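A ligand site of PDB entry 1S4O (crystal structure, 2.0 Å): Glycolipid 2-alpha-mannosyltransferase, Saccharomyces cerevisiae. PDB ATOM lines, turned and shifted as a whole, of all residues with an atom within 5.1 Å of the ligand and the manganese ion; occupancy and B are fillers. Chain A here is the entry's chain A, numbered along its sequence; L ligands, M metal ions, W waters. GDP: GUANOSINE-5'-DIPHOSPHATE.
Two residues have an atom within 4 Å of the manganese ion: Glu 153 and His 294.
Water W8 lies within hydrogen-bond range of O6 of the ligand (2.7 Å) and OD2 of Asp 67 (2.8 Å).
Water W5 bridges the side-chain carboxylate of Glu 153 (2.9 Å) and the side-chain amide nitrogen of Asn 233 (3.4 Å).
Water W3 bridges O1B of the ligand (2.7 Å) and OH of Tyr 126 (3.5 Å).
Water W6 lies within hydrogen-bond range of N7 of the ligand (2.9 Å), OG of Ser 125 (3.1 Å), N of Tyr 126 (3.2 Å) and NH1 of Arg 36 (3.3 Å).
Water W2 lies within hydrogen-bond range of O of Val 152, O3' of the ligand and N of Leu 34.
Water W7 bridges OG of Ser 125 (3.0 Å) and O6 of the ligand (3.1 Å).
Residues that only touch the ligand: Trp 96 (3.5 Å), Ser 125 (3.7 Å), Met 129 (3.6 Å) and Pro 154 (3.4 Å).
Along chain A the residues within 4 Å of the ligand span positions 34 to 294.
The manganese ion is bound by an oxygen (O1A) of the ligand (2.2 Å), the side-chain carboxylate (OE1) of Glu 153 (2.2 Å), an oxygen (O2B) of the ligand (2.3 Å), water W4 (2.3 Å), a ring nitrogen (NE2) of His 294 (2.3 Å) and water W10 (2.5 Å).
The guanidinium group (NH2) of Arg 151 is in salt-bridge range of the side-chain carboxylate (OE2) of Glu 153, 2.7 Å away.
ND1 of His 294 sits at hydrogen-bond distance from ND2 of Asn 233, 3.3 Å away.
The side-chain carboxylate (OD1) of Asp 67 sits close to the side-chain amide oxygen (OD1) of Asn 66, 3.2 Å away.
The side-chain carboxylate (OD2) of Asp 67 lies within hydrogen-bond range of the indole nitrogen (NE1) of Trp 96, at 3.4 Å.
NE of Arg 36 is in salt-bridge range of OE1 of Glu 39, 2.9 Å away.
The backbone carbonyl oxygen (O) of Val 35 lies close to the side-chain amide nitrogen (ND2) of Asn 66 (3.3 Å).
O of Leu 65 is in hydrogen-bond range of N of Val 35 (2.9 Å).
OD1 of Asp 67 lies within hydrogen-bond range of N1 of the ligand.
The side-chain hydroxyl (OH) of Tyr 120 is in hydrogen-bond range of an oxygen (O3B) of the ligand.
An oxygen (O3') of the ligand is in hydrogen-bond range of the backbone carbonyl oxygen of Leu 34.
The side-chain hydroxyl of Tyr 126 sits at hydrogen-bond distance from an oxygen (O1B) of the ligand (2.7 Å).
OE1 of Glu 39 is in hydrogen-bond range of O2' of the ligand, 2.8 Å away.
The side-chain amide oxygen (OD1) of Asn 66 lies within hydrogen-bond range of a nitrogen (N2) of the ligand.
The guanidinium group of Arg 36 lies within salt-bridge range of an oxygen (O2A) of the ligand (3.0 Å).
O of Val 35 sits at hydrogen-bond distance from N2 of the ligand, at 3.2 Å.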
ATOM      1  N   THR A  33       6.080 -10.833   4.933  1.00  0.00           N
ATOM      2  CA  THR A  33       6.055 -10.877   3.493  1.00  0.00           C
ATOM      3  C   THR A  33       7.128 -10.006   2.844  1.00  0.00           C
ATOM      4  O   THR A  33       7.193  -8.809   3.086  1.00  0.00           O
ATOM      5  CB  THR A  33       4.650 -10.437   2.964  1.00  0.00           C
ATOM      6  OG1 THR A  33       3.669 -11.442   3.303  1.00  0.00           O
ATOM      7  CG2 THR A  33       4.654 -10.260   1.461  1.00  0.00           C
ATOM      8  N   LEU A  34       8.022 -10.625   2.079  1.00  0.00           N
ATOM      9  CA  LEU A  34       9.035  -9.856   1.342  1.00  0.00           C
ATOM     10  C   LEU A  34       8.380  -9.739  -0.047  1.00  0.00           C
ATOM     11  O   LEU A  34       8.054 -10.758  -0.642  1.00  0.00           O
ATOM     12  CB  LEU A  34      10.356 -10.631   1.257  1.00  0.00           C
ATOM     13  CG  LEU A  34      11.328 -10.100   0.185  1.00  0.00           C
ATOM     14  CD1 LEU A  34      11.962  -8.802   0.690  1.00  0.00           C
ATOM     15  CD2 LEU A  34      12.431 -11.144  -0.129  1.00  0.00           C
ATOM     16  N   VAL A  35       8.182  -8.529  -0.552  1.00  0.00           N
ATOM     17  CA  VAL A  35       7.488  -8.352  -1.840  1.00  0.00           C
ATOM     18  C   VAL A  35       7.873  -7.092  -2.622  1.00  0.00           C
ATOM     19  O   VAL A  35       8.341  -6.110  -2.039  1.00  0.00           O
ATOM     20  CB  VAL A  35       5.956  -8.331  -1.585  1.00  0.00           C
ATOM     21  CG1 VAL A  35       5.603  -7.171  -0.629  1.00  0.00           C
ATOM     22  CG2 VAL A  35       5.193  -8.196  -2.908  1.00  0.00           C
ATOM     23  N   ARG A  36       7.652  -7.121  -3.943  1.00  0.00           N
ATOM     24  CA  ARG A  36       7.939  -5.982  -4.829  1.00  0.00           C
ATOM     25  C   ARG A  36       6.691  -5.106  -5.073  1.00  0.00           C
ATOM     26  O   ARG A  36       5.545  -5.586  -5.007  1.00  0.00           O
ATOM     27  CB  ARG A  36       8.468  -6.492  -6.169  1.00  0.00           C
ATOM     28  CG  ARG A  36       9.889  -7.021  -6.089  1.00  0.00           C
ATOM     29  CD  ARG A  36      10.246  -7.905  -7.291  1.00  0.00           C
ATOM     30  NE  ARG A  36       9.547  -9.185  -7.220  1.00  0.00           N
ATOM     31  CZ  ARG A  36       9.926 -10.294  -7.852  1.00  0.00           C
ATOM     32  NH1 ARG A  36      11.024 -10.279  -8.609  1.00  0.00           N
ATOM     33  NH2 ARG A  36       9.231 -11.430  -7.678  1.00  0.00           N
ATOM     34  N   GLU A  39       4.020  -6.141  -7.676  1.00  0.00           N
ATOM     35  CA  GLU A  39       3.324  -7.412  -7.446  1.00  0.00           C
ATOM     36  C   GLU A  39       2.100  -7.153  -6.573  1.00  0.00           C
ATOM     37  O   GLU A  39       1.570  -8.082  -5.936  1.00  0.00           O
ATOM     38  CB  GLU A  39       4.237  -8.405  -6.728  1.00  0.00           C
ATOM     39  CG  GLU A  39       5.453  -8.830  -7.524  1.00  0.00           C
ATOM     40  CD  GLU A  39       6.325  -9.783  -6.748  1.00  0.00           C
ATOM     41  OE1 GLU A  39       7.010  -9.357  -5.802  1.00  0.00           O
ATOM     42  OE2 GLU A  39       6.297 -10.973  -7.092  1.00  0.00           O
ATOM     43  N   LEU A  65       8.042  -6.386   3.860  1.00  0.00           N
ATOM     44  CA  LEU A  65       9.422  -5.977   3.598  1.00  0.00           C
ATOM     45  C   LEU A  65       9.730  -5.814   2.109  1.00  0.00           C
ATOM     46  O   LEU A  65       9.232  -6.559   1.276  1.00  0.00           O
ATOM     47  CB  LEU A  65      10.385  -7.013   4.188  1.00  0.00           C
ATOM     48  CG  LEU A  65      10.194  -7.420   5.657  1.00  0.00           C
ATOM     49  CD1 LEU A  65      11.279  -8.405   6.056  1.00  0.00           C
ATOM     50  CD2 LEU A  65      10.276  -6.185   6.543  1.00  0.00           C
ATOM     51  N   ASN A  66      10.573  -4.838   1.783  1.00  0.00           N
ATOM     52  CA  ASN A  66      10.958  -4.615   0.393  1.00  0.00           C
ATOM     53  C   ASN A  66      12.411  -4.133   0.360  1.00  0.00           C
ATOM     54  O   ASN A  66      12.843  -3.416   1.276  1.00  0.00           O
ATOM     55  CB  ASN A  66      10.030  -3.570  -0.242  1.00  0.00           C
ATOM     56  CG  ASN A  66      10.180  -3.499  -1.780  1.00  0.00           C
ATOM     57  OD1 ASN A  66      11.175  -3.932  -2.331  1.00  0.00           O
ATOM     58  ND2 ASN A  66       9.176  -2.909  -2.450  1.00  0.00           N
ATOM     59  N   ASP A  67      13.179  -4.541  -0.656  1.00  0.00           N
ATOM     60  CA  ASP A  67      14.561  -4.092  -0.742  1.00  0.00           C
ATOM     61  C   ASP A  67      14.583  -2.640  -1.232  1.00  0.00           C
ATOM     62  O   ASP A  67      15.580  -1.941  -1.072  1.00  0.00           O
ATOM     63  CB  ASP A  67      15.386  -5.020  -1.661  1.00  0.00           C
ATOM     64  CG  ASP A  67      14.892  -5.037  -3.101  1.00  0.00           C
ATOM     65  OD1 ASP A  67      13.758  -5.488  -3.369  1.00  0.00           O
ATOM     66  OD2 ASP A  67      15.670  -4.612  -3.979  1.00  0.00           O
ATOM     67  N   TRP A  96      21.260  -7.069   1.402  1.00  0.00           N
ATOM     68  CA  TRP A  96      20.860  -7.164   0.003  1.00  0.00           C
ATOM     69  C   TRP A  96      21.909  -6.443  -0.829  1.00  0.00           C
ATOM     70  O   TRP A  96      21.645  -5.369  -1.359  1.00  0.00           O
ATOM     71  CB  TRP A  96      19.517  -6.454  -0.211  1.00  0.00           C
ATOM     72  CG  TRP A  96      18.797  -6.812  -1.478  1.00  0.00           C
ATOM     73  CD1 TRP A  96      19.044  -6.351  -2.736  1.00  0.00           C
ATOM     74  CD2 TRP A  96      17.684  -7.709  -1.587  1.00  0.00           C
ATOM     75  NE1 TRP A  96      18.142  -6.898  -3.627  1.00  0.00           N
ATOM     76  CE2 TRP A  96      17.300  -7.728  -2.950  1.00  0.00           C
ATOM     77  CE3 TRP A  96      16.979  -8.490  -0.667  1.00  0.00           C
ATOM     78  CZ2 TRP A  96      16.223  -8.495  -3.402  1.00  0.00           C
ATOM     79  CZ3 TRP A  96      15.907  -9.248  -1.115  1.00  0.00           C
ATOM     80  CH2 TRP A  96      15.545  -9.243  -2.481  1.00  0.00           C
ATOM     81  N   TYR A 120      15.294 -18.586 -13.236  1.00  0.00           N
ATOM     82  CA  TYR A 120      15.996 -17.525 -12.540  1.00  0.00           C
ATOM     83  C   TYR A 120      17.507 -17.667 -12.684  1.00  0.00           C
ATOM     84  O   TYR A 120      18.282 -16.988 -11.972  1.00  0.00           O
ATOM     85  CB  TYR A 120      15.624 -17.502 -11.064  1.00  0.00           C
ATOM     86  CG  TYR A 120      14.153 -17.409 -10.804  1.00  0.00           C
ATOM     87  CD1 TYR A 120      13.389 -16.404 -11.388  1.00  0.00           C
ATOM     88  CD2 TYR A 120      13.513 -18.320  -9.978  1.00  0.00           C
ATOM     89  CE1 TYR A 120      12.033 -16.303 -11.148  1.00  0.00           C
ATOM     90  CE2 TYR A 120      12.148 -18.238  -9.735  1.00  0.00           C
ATOM     91  CZ  TYR A 120      11.420 -17.230 -10.322  1.00  0.00           C
ATOM     92  OH  TYR A 120      10.071 -17.153 -10.094  1.00  0.00           O
ATOM     93  N   SER A 125      18.728 -10.216  -9.045  1.00  0.00           N
ATOM     94  CA  SER A 125      17.904  -9.962  -7.874  1.00  0.00           C
ATOM     95  C   SER A 125      17.403 -11.224  -7.180  1.00  0.00           C
ATOM     96  O   SER A 125      17.276 -11.254  -5.960  1.00  0.00           O
ATOM     97  CB  SER A 125      16.702  -9.060  -8.223  1.00  0.00           C
ATOM     98  OG  SER A 125      15.895  -9.656  -9.205  1.00  0.00           O
ATOM     99  N   TYR A 126      17.100 -12.268  -7.936  1.00  0.00           N
ATOM    100  CA  TYR A 126      16.608 -13.499  -7.328  1.00  0.00           C
ATOM    101  C   TYR A 126      17.607 -14.119  -6.337  1.00  0.00           C
ATOM    102  O   TYR A 126      17.209 -14.659  -5.290  1.00  0.00           O
ATOM    103  CB  TYR A 126      16.273 -14.517  -8.403  1.00  0.00           C
ATOM    104  CG  TYR A 126      15.530 -15.710  -7.860  1.00  0.00           C
ATOM    105  CD1 TYR A 126      14.149 -15.652  -7.627  1.00  0.00           C
ATOM    106  CD2 TYR A 126      16.198 -16.888  -7.562  1.00  0.00           C
ATOM    107  CE1 TYR A 126      13.464 -16.732  -7.113  1.00  0.00           C
ATOM    108  CE2 TYR A 126      15.517 -17.984  -7.046  1.00  0.00           C
ATOM    109  CZ  TYR A 126      14.159 -17.898  -6.824  1.00  0.00           C
ATOM    110  OH  TYR A 126      13.473 -19.001  -6.378  1.00  0.00           O
ATOM    111  N   MET A 129      17.632 -12.306  -3.125  1.00  0.00           N
ATOM    112  CA  MET A 129      16.422 -12.669  -2.390  1.00  0.00           C
ATOM    113  C   MET A 129      16.627 -14.000  -1.632  1.00  0.00           C
ATOM    114  O   MET A 129      16.265 -14.107  -0.468  1.00  0.00           O
ATOM    115  CB  MET A 129      15.238 -12.784  -3.361  1.00  0.00           C
ATOM    116  CG  MET A 129      13.884 -13.175  -2.757  1.00  0.00           C
ATOM    117  SD  MET A 129      13.643 -14.951  -2.390  1.00  0.00           S
ATOM    118  CE  MET A 129      13.600 -15.688  -4.021  1.00  0.00           C
ATOM    119  N   GLN A 133      16.381 -14.425   2.408  1.00  0.00           N
ATOM    120  CA  GLN A 133      15.478 -15.308   3.122  1.00  0.00           C
ATOM    121  C   GLN A 133      16.262 -16.341   3.958  1.00  0.00           C
ATOM    122  O   GLN A 133      15.763 -16.860   4.959  1.00  0.00           O
ATOM    123  CB  GLN A 133      14.554 -16.010   2.124  1.00  0.00           C
ATOM    124  CG  GLN A 133      13.668 -15.059   1.281  1.00  0.00           C
ATOM    125  CD  GLN A 133      12.477 -14.480   2.061  1.00  0.00           C
ATOM    126  OE1 GLN A 133      11.446 -14.149   1.480  1.00  0.00           O
ATOM    127  NE2 GLN A 133      12.620 -14.350   3.384  1.00  0.00           N
ATOM    128  N   ARG A 151       5.314 -16.982   6.927  1.00  0.00           N
ATOM    129  CA  ARG A 151       5.644 -16.363   5.647  1.00  0.00           C
ATOM    130  C   ARG A 151       4.514 -16.491   4.618  1.00  0.00           C
ATOM    131  O   ARG A 151       3.934 -17.571   4.448  1.00  0.00           O
ATOM    132  CB  ARG A 151       6.916 -16.984   5.084  1.00  0.00           C
ATOM    133  CG  ARG A 151       7.328 -16.452   3.729  1.00  0.00           C
ATOM    134  CD  ARG A 151       8.710 -16.947   3.361  1.00  0.00           C
ATOM    135  NE  ARG A 151       8.994 -16.806   1.931  1.00  0.00           N
ATOM    136  CZ  ARG A 151      10.139 -17.198   1.382  1.00  0.00           C
ATOM    137  NH1 ARG A 151      11.078 -17.744   2.137  1.00  0.00           N
ATOM    138  NH2 ARG A 151      10.329 -17.069   0.069  1.00  0.00           N
ATOM    139  N   VAL A 152       4.199 -15.383   3.965  1.00  0.00           N
ATOM    140  CA  VAL A 152       3.155 -15.339   2.966  1.00  0.00           C
ATOM    141  C   VAL A 152       3.663 -14.673   1.689  1.00  0.00           C
ATOM    142  O   VAL A 152       4.231 -13.568   1.727  1.00  0.00           O
ATOM    143  CB  VAL A 152       1.922 -14.558   3.480  1.00  0.00           C
ATOM    144  CG1 VAL A 152       0.884 -14.420   2.369  1.00  0.00           C
ATOM    145  CG2 VAL A 152       1.319 -15.272   4.689  1.00  0.00           C
ATOM    146  N   GLU A 153       3.466 -15.325   0.553  1.00  0.00           N
ATOM    147  CA  GLU A 153       3.904 -14.731  -0.718  1.00  0.00           C
ATOM    148  C   GLU A 153       2.707 -14.285  -1.559  1.00  0.00           C
ATOM    149  O   GLU A 153       1.559 -14.661  -1.286  1.00  0.00           O
ATOM    150  CB  GLU A 153       4.740 -15.731  -1.539  1.00  0.00           C
ATOM    151  CG  GLU A 153       6.028 -16.208  -0.858  1.00  0.00           C
ATOM    152  CD  GLU A 153       7.005 -16.878  -1.814  1.00  0.00           C
ATOM    153  OE1 GLU A 153       6.687 -16.993  -3.020  1.00  0.00           O
ATOM    154  OE2 GLU A 153       8.106 -17.301  -1.365  1.00  0.00           O
ATOM    155  N   PRO A 154       2.956 -13.459  -2.572  1.00  0.00           N
ATOM    156  CA  PRO A 154       1.810 -13.045  -3.389  1.00  0.00           C
ATOM    157  C   PRO A 154       1.391 -14.190  -4.326  1.00  0.00           C
ATOM    158  O   PRO A 154       2.172 -15.127  -4.573  1.00  0.00           O
ATOM    159  CB  PRO A 154       2.335 -11.842  -4.160  1.00  0.00           C
ATOM    160  CG  PRO A 154       3.816 -12.119  -4.265  1.00  0.00           C
ATOM    161  CD  PRO A 154       4.172 -12.703  -2.925  1.00  0.00           C
ATOM    162  N   ASN A 233       8.000 -20.876   0.603  1.00  0.00           N
ATOM    163  CA  ASN A 233       6.960 -19.855   0.473  1.00  0.00           C
ATOM    164  C   ASN A 233       5.951 -20.030   1.601  1.00  0.00           C
ATOM    165  O   ASN A 233       5.317 -19.078   2.006  1.00  0.00           O
ATOM    166  CB  ASN A 233       6.286 -19.883  -0.930  1.00  0.00           C
ATOM    167  CG  ASN A 233       5.949 -21.282  -1.384  1.00  0.00           C
ATOM    168  OD1 ASN A 233       4.975 -21.881  -0.938  1.00  0.00           O
ATOM    169  ND2 ASN A 233       6.786 -21.819  -2.259  1.00  0.00           N
ATOM    170  N   HIS A 294       0.642 -22.530  -4.056  1.00  0.00           N
ATOM    171  CA  HIS A 294       1.673 -21.571  -4.422  1.00  0.00           C
ATOM    172  C   HIS A 294       1.924 -22.161  -5.804  1.00  0.00           C
ATOM    173  O   HIS A 294       2.316 -23.323  -5.903  1.00  0.00           O
ATOM    174  CB  HIS A 294       2.929 -21.664  -3.550  1.00  0.00           C
ATOM    175  CG  HIS A 294       4.100 -20.922  -4.106  1.00  0.00           C
ATOM    176  ND1 HIS A 294       4.998 -21.493  -4.993  1.00  0.00           N
ATOM    177  CD2 HIS A 294       4.485 -19.631  -3.955  1.00  0.00           C
ATOM    178  CE1 HIS A 294       5.888 -20.583  -5.356  1.00  0.00           C
ATOM    179  NE2 HIS A 294       5.606 -19.452  -4.747  1.00  0.00           N
HETATM  180  PB  GDP L   1       9.536 -18.172  -6.580  1.00  0.00           P
HETATM  181  O1B GDP L   1      10.795 -18.939  -6.553  1.00  0.00           O
HETATM  182  O2B GDP L   1       8.548 -18.588  -5.482  1.00  0.00           O
HETATM  183  O3B GDP L   1       8.887 -18.156  -7.974  1.00  0.00           O
HETATM  184  O3A GDP L   1       9.954 -16.601  -6.240  1.00  0.00           O
HETATM  185  PA  GDP L   1       9.093 -15.308  -6.056  1.00  0.00           P
HETATM  186  O1A GDP L   1       7.670 -15.563  -5.703  1.00  0.00           O
HETATM  187  O2A GDP L   1       9.314 -14.423  -7.260  1.00  0.00           O
HETATM  188  O5' GDP L   1       9.829 -14.598  -4.809  1.00  0.00           O
HETATM  189  C5' GDP L   1       9.796 -15.178  -3.477  1.00  0.00           C
HETATM  190  C4' GDP L   1       9.267 -14.097  -2.540  1.00  0.00           C
HETATM  191  O4' GDP L   1      10.299 -13.083  -2.555  1.00  0.00           O
HETATM  192  C3' GDP L   1       7.961 -13.429  -3.013  1.00  0.00           C
HETATM  193  O3' GDP L   1       7.300 -13.052  -1.756  1.00  0.00           O
HETATM  194  C2' GDP L   1       8.432 -12.194  -3.751  1.00  0.00           C
HETATM  195  O2' GDP L   1       7.467 -11.182  -3.759  1.00  0.00           O
HETATM  196  C1' GDP L   1       9.757 -11.876  -3.032  1.00  0.00           C
HETATM  197  N9  GDP L   1      10.837 -11.262  -3.987  1.00  0.00           N
HETATM  198  C8  GDP L   1      11.436 -11.884  -5.044  1.00  0.00           C
HETATM  199  N7  GDP L   1      12.303 -11.070  -5.630  1.00  0.00           N
HETATM  200  C5  GDP L   1      12.255  -9.888  -4.900  1.00  0.00           C
HETATM  201  C6  GDP L   1      12.977  -8.693  -5.049  1.00  0.00           C
HETATM  202  O6  GDP L   1      13.832  -8.475  -5.914  1.00  0.00           O
HETATM  203  N1  GDP L   1      12.635  -7.711  -4.104  1.00  0.00           N
HETATM  204  C2  GDP L   1      11.676  -7.901  -3.111  1.00  0.00           C
HETATM  205  N2  GDP L   1      11.413  -6.883  -2.258  1.00  0.00           N
HETATM  206  N3  GDP L   1      11.002  -9.061  -2.974  1.00  0.00           N
HETATM  207  C4  GDP L   1      11.345  -9.989  -3.893  1.00  0.00           C
HETATM  208 MN    MN M   1       6.611 -17.407  -5.195  1.00  0.00          MN
HETATM  209  O   HOH W   1       6.017 -13.513  -6.131  1.00  0.00           O
HETATM  210  O   HOH W   2       7.120 -13.558   1.185  1.00  0.00           O
HETATM  211  O   HOH W   3      11.130 -20.950  -4.754  1.00  0.00           O
HETATM  212  O   HOH W   4       4.556 -16.432  -5.599  1.00  0.00           O
HETATM  213  O   HOH W   5       9.128 -19.445  -2.981  1.00  0.00           O
HETATM  214  O   HOH W   6      13.923 -11.689  -7.934  1.00  0.00           O
HETATM  215  O   HOH W   7      13.633  -7.783  -8.921  1.00  0.00           O
HETATM  216  O   HOH W   8      15.257  -6.254  -6.257  1.00  0.00           O
HETATM  217  O   HOH W   9       6.860 -14.617  -9.064  1.00  0.00           O
HETATM  218  O   HOH W  10       6.380 -17.473  -7.663  1.00  0.00           O
